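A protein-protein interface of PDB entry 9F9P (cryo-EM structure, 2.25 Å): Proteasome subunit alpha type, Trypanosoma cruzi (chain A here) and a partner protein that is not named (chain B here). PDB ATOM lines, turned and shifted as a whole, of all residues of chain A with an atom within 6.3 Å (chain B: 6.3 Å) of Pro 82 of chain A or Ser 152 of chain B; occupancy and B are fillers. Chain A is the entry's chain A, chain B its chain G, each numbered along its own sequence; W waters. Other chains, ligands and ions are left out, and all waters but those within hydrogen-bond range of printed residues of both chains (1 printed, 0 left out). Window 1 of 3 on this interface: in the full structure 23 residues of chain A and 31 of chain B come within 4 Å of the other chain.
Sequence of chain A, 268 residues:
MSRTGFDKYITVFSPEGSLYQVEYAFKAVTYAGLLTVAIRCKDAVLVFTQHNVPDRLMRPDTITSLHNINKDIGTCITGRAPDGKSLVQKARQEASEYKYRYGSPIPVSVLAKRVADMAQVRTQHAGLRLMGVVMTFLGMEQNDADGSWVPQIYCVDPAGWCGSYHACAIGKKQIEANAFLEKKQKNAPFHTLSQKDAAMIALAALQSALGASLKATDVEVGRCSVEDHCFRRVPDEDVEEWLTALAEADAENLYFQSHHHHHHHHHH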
ATOM      1  N   GLY A  79     -36.308  16.498  12.860  1.00  0.00           N
ATOM      2  CA  GLY A  79     -35.904  17.873  13.123  1.00  0.00           C
ATOM      3  C   GLY A  79     -34.572  18.002  13.859  1.00  0.00           C
ATOM      4  O   GLY A  79     -33.686  17.184  13.716  1.00  0.00           O
ATOM      5  N   ARG A  80     -34.427  19.026  14.668  1.00  0.00           N
ATOM      6  CA  ARG A  80     -33.168  19.324  15.330  1.00  0.00           C
ATOM      7  C   ARG A  80     -32.807  18.257  16.382  1.00  0.00           C
ATOM      8  O   ARG A  80     -33.454  18.136  17.411  1.00  0.00           O
ATOM      9  CB  ARG A  80     -33.328  20.727  15.908  1.00  0.00           C
ATOM     10  CG  ARG A  80     -32.039  21.366  16.383  1.00  0.00           C
ATOM     11  CD  ARG A  80     -32.215  22.777  16.971  1.00  0.00           C
ATOM     12  NE  ARG A  80     -30.992  23.215  17.665  1.00  0.00           N
ATOM     13  CZ  ARG A  80     -29.953  23.767  17.056  1.00  0.00           C
ATOM     14  NH1 ARG A  80     -30.022  24.047  15.778  1.00  0.00           N
ATOM     15  NH2 ARG A  80     -28.843  24.046  17.717  1.00  0.00           N
ATOM     16  N   ALA A  81     -31.751  17.473  16.135  1.00  0.00           N
ATOM     17  CA  ALA A  81     -31.615  16.188  16.796  1.00  0.00           C
ATOM     18  C   ALA A  81     -31.508  16.333  18.314  1.00  0.00           C
ATOM     19  O   ALA A  81     -32.119  15.580  19.072  1.00  0.00           O
ATOM     20  CB  ALA A  81     -30.416  15.476  16.227  1.00  0.00           C
ATOM     21  N   PRO A  82     -30.672  17.231  18.852  1.00  0.00           N
ATOM     22  CA  PRO A  82     -30.543  17.303  20.302  1.00  0.00           C
ATOM     23  C   PRO A  82     -31.751  17.836  21.041  1.00  0.00           C
ATOM     24  O   PRO A  82     -31.920  17.542  22.229  1.00  0.00           O
ATOM     25  CB  PRO A  82     -29.331  18.183  20.527  1.00  0.00           C
ATOM     26  CG  PRO A  82     -29.139  18.937  19.215  1.00  0.00           C
ATOM     27  CD  PRO A  82     -29.656  18.018  18.133  1.00  0.00           C
ATOM     28  N   ASP A  83     -32.577  18.603  20.325  1.00  0.00           N
ATOM     29  CA  ASP A  83     -33.828  19.068  20.867  1.00  0.00           C
ATOM     30  C   ASP A  83     -34.725  17.863  21.116  1.00  0.00           C
ATOM     31  O   ASP A  83     -35.332  17.743  22.177  1.00  0.00           O
ATOM     32  CB  ASP A  83     -34.518  20.053  19.931  1.00  0.00           C
ATOM     33  CG  ASP A  83     -34.037  21.498  19.929  1.00  0.00           C
ATOM     34  OD1 ASP A  83     -32.908  21.814  20.515  1.00  0.00           O
ATOM     35  OD2 ASP A  83     -34.740  22.307  19.266  1.00  0.00           O
ATOM     36  N   GLY A  84     -34.798  16.990  20.111  1.00  0.00           N
ATOM     37  CA  GLY A  84     -35.547  15.747  20.205  1.00  0.00           C
ATOM     38  C   GLY A  84     -35.065  14.853  21.349  1.00  0.00           C
ATOM     39  O   GLY A  84     -35.918  14.345  22.055  1.00  0.00           O
ATOM     40  N   LYS A  85     -33.733  14.707  21.568  1.00  0.00           N
ATOM     41  CA  LYS A  85     -33.269  13.939  22.720  1.00  0.00           C
ATOM     42  C   LYS A  85     -33.680  14.579  24.037  1.00  0.00           C
ATOM     43  O   LYS A  85     -33.947  13.864  24.994  1.00  0.00           O
ATOM     44  CB  LYS A  85     -31.769  13.689  22.845  1.00  0.00           C
ATOM     45  CG  LYS A  85     -31.080  13.311  21.559  1.00  0.00           C
ATOM     46  CD  LYS A  85     -31.017  11.829  21.257  1.00  0.00           C
ATOM     47  CE  LYS A  85     -30.408  11.587  19.881  1.00  0.00           C
ATOM     48  NZ  LYS A  85     -29.678  10.294  19.822  1.00  0.00           N
ATOM     49  N   SER A  86     -33.792  15.890  24.131  1.00  0.00           N
ATOM     50  CA  SER A  86     -34.275  16.404  25.389  1.00  0.00           C
ATOM     51  C   SER A  86     -35.727  16.017  25.627  1.00  0.00           C
ATOM     52  O   SER A  86     -36.115  15.870  26.783  1.00  0.00           O
ATOM     53  CB  SER A  86     -34.050  17.896  25.587  1.00  0.00           C
ATOM     54  OG  SER A  86     -34.955  18.654  24.844  1.00  0.00           O
ATOM     55  N   LEU A  87     -36.552  15.906  24.577  1.00  0.00           N
ATOM     56  CA  LEU A  87     -37.938  15.522  24.786  1.00  0.00           C
ATOM     57  C   LEU A  87     -38.098  14.019  25.094  1.00  0.00           C
ATOM     58  O   LEU A  87     -38.994  13.667  25.855  1.00  0.00           O
ATOM     59  CB  LEU A  87     -38.754  15.911  23.564  1.00  0.00           C
ATOM     60  CG  LEU A  87     -39.067  17.401  23.441  1.00  0.00           C
ATOM     61  CD1 LEU A  87     -39.952  17.662  22.245  1.00  0.00           C
ATOM     62  CD2 LEU A  87     -39.742  17.931  24.697  1.00  0.00           C
ATOM     63  N   MET A 131     -38.748  23.791  21.045  1.00  0.00           N
ATOM     64  CA  MET A 131     -37.972  22.698  20.485  1.00  0.00           C
ATOM     65  C   MET A 131     -38.394  22.450  19.038  1.00  0.00           C
ATOM     66  O   MET A 131     -39.556  22.164  18.772  1.00  0.00           O
ATOM     67  CB  MET A 131     -38.185  21.424  21.304  1.00  0.00           C
ATOM     68  CG  MET A 131     -37.791  21.516  22.782  1.00  0.00           C
ATOM     69  SD  MET A 131     -35.963  21.469  23.088  1.00  0.00           S
ATOM     70  CE  MET A 131     -35.576  23.229  22.999  1.00  0.00           C
ATOM     71  N   VAL B  22     -25.467  29.396  18.425  1.00  0.00           N
ATOM     72  CA  VAL B  22     -24.824  28.095  18.516  1.00  0.00           C
ATOM     73  C   VAL B  22     -23.830  27.919  17.379  1.00  0.00           C
ATOM     74  O   VAL B  22     -22.798  27.301  17.560  1.00  0.00           O
ATOM     75  CB  VAL B  22     -25.828  26.938  18.542  1.00  0.00           C
ATOM     76  CG1 VAL B  22     -25.133  25.599  18.455  1.00  0.00           C
ATOM     77  CG2 VAL B  22     -26.675  26.950  19.793  1.00  0.00           C
ATOM     78  N   CYS B  26     -19.625  27.313  17.561  1.00  0.00           N
ATOM     79  CA  CYS B  26     -18.937  26.278  16.797  1.00  0.00           C
ATOM     80  C   CYS B  26     -17.723  26.839  16.062  1.00  0.00           C
ATOM     81  O   CYS B  26     -16.760  26.124  15.833  1.00  0.00           O
ATOM     82  CB  CYS B  26     -19.866  25.623  15.786  1.00  0.00           C
ATOM     83  SG  CYS B  26     -21.165  24.636  16.591  1.00  0.00           S
ATOM     84  N   GLY B 115     -23.791  15.367  26.330  1.00  0.00           N
ATOM     85  CA  GLY B 115     -24.693  15.979  25.353  1.00  0.00           C
ATOM     86  C   GLY B 115     -25.887  16.712  25.957  1.00  0.00           C
ATOM     87  O   GLY B 115     -26.165  17.834  25.578  1.00  0.00           O
ATOM     88  N   MET B 118     -24.747  19.964  27.752  1.00  0.00           N
ATOM     89  CA  MET B 118     -24.373  20.993  26.808  1.00  0.00           C
ATOM     90  C   MET B 118     -25.588  21.586  26.097  1.00  0.00           C
ATOM     91  O   MET B 118     -25.644  22.783  25.881  1.00  0.00           O
ATOM     92  CB  MET B 118     -23.384  20.446  25.780  1.00  0.00           C
ATOM     93  CG  MET B 118     -21.975  20.237  26.432  1.00  0.00           C
ATOM     94  SD  MET B 118     -20.674  19.451  25.388  1.00  0.00           S
ATOM     95  CE  MET B 118     -20.001  20.880  24.559  1.00  0.00           C
ATOM     96  N   HIS B 119     -26.573  20.754  25.749  1.00  0.00           N
ATOM     97  CA  HIS B 119     -27.777  21.221  25.074  1.00  0.00           C
ATOM     98  C   HIS B 119     -28.560  22.223  25.904  1.00  0.00           C
ATOM     99  O   HIS B 119     -29.144  23.144  25.347  1.00  0.00           O
ATOM    100  CB  HIS B 119     -28.717  20.055  24.732  1.00  0.00           C
ATOM    101  CG  HIS B 119     -30.031  20.436  24.157  1.00  0.00           C
ATOM    102  ND1 HIS B 119     -31.173  20.561  24.931  1.00  0.00           N
ATOM    103  CD2 HIS B 119     -30.358  20.800  22.902  1.00  0.00           C
ATOM    104  CE1 HIS B 119     -32.167  20.996  24.143  1.00  0.00           C
ATOM    105  NE2 HIS B 119     -31.690  21.162  22.901  1.00  0.00           N
ATOM    106  N   THR B 122     -28.230  25.875  25.344  1.00  0.00           N
ATOM    107  CA  THR B 122     -28.671  26.454  24.076  1.00  0.00           C
ATOM    108  C   THR B 122     -30.160  26.841  24.085  1.00  0.00           C
ATOM    109  O   THR B 122     -30.741  27.059  23.030  1.00  0.00           O
ATOM    110  CB  THR B 122     -28.469  25.463  22.925  1.00  0.00           C
ATOM    111  OG1 THR B 122     -29.320  24.319  23.027  1.00  0.00           O
ATOM    112  CG2 THR B 122     -27.051  24.936  22.900  1.00  0.00           C
ATOM    113  N   PHE B 130     -21.566  26.540  25.250  1.00  0.00           N
ATOM    114  CA  PHE B 130     -20.160  26.255  25.481  1.00  0.00           C
ATOM    115  C   PHE B 130     -19.383  26.418  24.192  1.00  0.00           C
ATOM    116  O   PHE B 130     -19.892  26.124  23.134  1.00  0.00           O
ATOM    117  CB  PHE B 130     -19.950  24.835  25.977  1.00  0.00           C
ATOM    118  CG  PHE B 130     -20.395  24.589  27.387  1.00  0.00           C
ATOM    119  CD1 PHE B 130     -21.565  23.914  27.654  1.00  0.00           C
ATOM    120  CD2 PHE B 130     -19.626  24.992  28.445  1.00  0.00           C
ATOM    121  CE1 PHE B 130     -21.965  23.667  28.954  1.00  0.00           C
ATOM    122  CE2 PHE B 130     -20.024  24.769  29.757  1.00  0.00           C
ATOM    123  CZ  PHE B 130     -21.186  24.096  30.010  1.00  0.00           C
ATOM    124  N   ASP B 150     -20.681  18.121  20.540  1.00  0.00           N
ATOM    125  CA  ASP B 150     -20.349  19.495  20.160  1.00  0.00           C
ATOM    126  C   ASP B 150     -21.190  20.538  20.915  1.00  0.00           C
ATOM    127  O   ASP B 150     -21.928  20.206  21.825  1.00  0.00           O
ATOM    128  CB  ASP B 150     -20.396  19.648  18.648  1.00  0.00           C
ATOM    129  CG  ASP B 150     -21.800  19.516  18.134  1.00  0.00           C
ATOM    130  OD1 ASP B 150     -22.038  18.580  17.316  1.00  0.00           O
ATOM    131  OD2 ASP B 150     -22.655  20.332  18.563  1.00  0.00           O
ATOM    132  N   PRO B 151     -20.989  21.855  20.668  1.00  0.00           N
ATOM    133  CA  PRO B 151     -21.736  22.909  21.356  1.00  0.00           C
ATOM    134  C   PRO B 151     -23.258  22.892  21.203  1.00  0.00           C
ATOM    135  O   PRO B 151     -23.956  23.390  22.085  1.00  0.00           O
ATOM    136  CB  PRO B 151     -21.210  24.209  20.728  1.00  0.00           C
ATOM    137  CG  PRO B 151     -19.812  23.838  20.247  1.00  0.00           C
ATOM    138  CD  PRO B 151     -19.975  22.420  19.759  1.00  0.00           C
ATOM    139  N   SER B 152     -23.770  22.304  20.122  1.00  0.00           N
ATOM    140  CA  SER B 152     -25.199  22.132  19.995  1.00  0.00           C
ATOM    141  C   SER B 152     -25.745  21.062  20.935  1.00  0.00           C
ATOM    142  O   SER B 152     -26.965  20.960  21.065  1.00  0.00           O
ATOM    143  CB  SER B 152     -25.592  21.807  18.577  1.00  0.00           C
ATOM    144  OG  SER B 152     -25.253  20.477  18.245  1.00  0.00           O
ATOM    145  N   GLY B 153     -24.886  20.211  21.501  1.00  0.00           N
ATOM    146  CA  GLY B 153     -25.317  19.057  22.293  1.00  0.00           C
ATOM    147  C   GLY B 153     -25.545  17.783  21.483  1.00  0.00           C
ATOM    148  O   GLY B 153     -25.957  16.760  22.013  1.00  0.00           O
ATOM    149  N   THR B 154     -25.235  17.837  20.196  1.00  0.00           N
ATOM    150  CA  THR B 154     -25.293  16.667  19.342  1.00  0.00           C
ATOM    151  C   THR B 154     -24.160  15.684  19.665  1.00  0.00           C
ATOM    152  O   THR B 154     -23.030  16.081  19.799  1.00  0.00           O
ATOM    153  CB  THR B 154     -25.162  17.106  17.883  1.00  0.00           C
ATOM    154  OG1 THR B 154     -26.166  18.087  17.597  1.00  0.00           O
ATOM    155  CG2 THR B 154     -25.290  15.935  16.929  1.00  0.00           C
ATOM    156  N   VAL B 155     -24.460  14.386  19.707  1.00  0.00           N
ATOM    157  CA  VAL B 155     -23.526  13.365  20.146  1.00  0.00           C
ATOM    158  C   VAL B 155     -23.433  12.273  19.093  1.00  0.00           C
ATOM    159  O   VAL B 155     -24.490  11.721  18.781  1.00  0.00           O
ATOM    160  CB  VAL B 155     -24.011  12.722  21.451  1.00  0.00           C
ATOM    161  CG1 VAL B 155     -23.148  11.534  21.830  1.00  0.00           C
ATOM    162  CG2 VAL B 155     -24.015  13.708  22.587  1.00  0.00           C
HETATM  163  O   HOH W   1     -28.912  23.104  20.636  1.00  0.00           O
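The side-chain hydroxyl (OG1) of Thr 122 of chain B is in hydrogen-bond range of the backbone carbonyl oxygen (O) of His 119 of chain B (2.6 Å).
OD2 of Asp 150 of chain B sits at hydrogen-bond distance from OG of Ser 152 of chain B.
OG of Ser 86 of chain A lies within hydrogen-bond range of SD of Met 131 of chain A (3.5 Å).
OD1 of Asp 83 of chain A lies within salt-bridge range of NE of Arg 80 of chain A (3.7 Å).
O of Asp 83 of chain A is in hydrogen-bond range of OG of Ser 86 of chain A (2.8 Å).
OG1 of Thr 154 of chain B sits at hydrogen-bond distance from OG of Ser 152 of chain B.
The side-chain carboxylate of Asp 83 of chain A is in hydrogen-bond range of a ring nitrogen (NE2) of His 119 of chain B, 2.8 Å away.
Printed residues of chain B that touch a printed residue of chain A: His 119, Ser 152, Gly 153 and Thr 154.
Hydrophobic or aromatic side chains of chain A within 4 Å of the printed part of chain B: Pro 82 and Met 131.
Along chain A the printed residues that touch a printed residue of chain B span positions 82 to 131.
Among the printed residues, no Asp or Glu carboxylate lies within 4 Å of a Lys or Arg side-chain nitrogen of the other chain.
Pro 82 of chain A touches just these residues of chain B: His 119 (3.7 Å), Ser 152 (3.5 Å), Gly 153 (3.9 Å) and Thr 154 (3.5 Å).
Of the printed residues of chain B, Asp 83 of chain A touches His 119.
Lys 85 of chain A touches none of the printed residues of chain B.
Of the printed residues of chain B, Ser 86 of chain A touches His 119.
Printed residues of chain B within 4 Å of Met 131 of chain A: His 119 (3.97 Å).
Ser 152 of chain B touches just one residue of chain A: Pro 82 (3.5 Å).
Of the printed residues of chain A, Gly 153 of chain B touches Pro 82 (3.9 Å).
Printed residues of chain A within 4 Å of Thr 154 of chain B: Pro 82.
The nearest residue of chain B that does not touch Pro 82 of chain A is Gly 115 of chain B (6.0 Å).
Water W1 lies within hydrogen-bond range of OG1 of Thr 122 of chain B (2.7 Å), O of Ser 152 of chain B (2.9 Å) and NH2 of Arg 80 of chain A (3.1 Å).
Among the printed residues, merely in contact across the chains: Pro 82 of chain A with His 119 of chain B (3.7 Å), Pro 82 of chain A with Ser 152 of chain B (3.5 Å), Pro 82 of chain A with Gly 153 of chain B (3.9 Å), Pro 82 of chain A with Thr 154 of chain B (3.5 Å), Ser 86 of chain A with His 119 of chain B (3.7 Å) and Met 131 of chain A with His 119 of chain B (3.97 Å).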
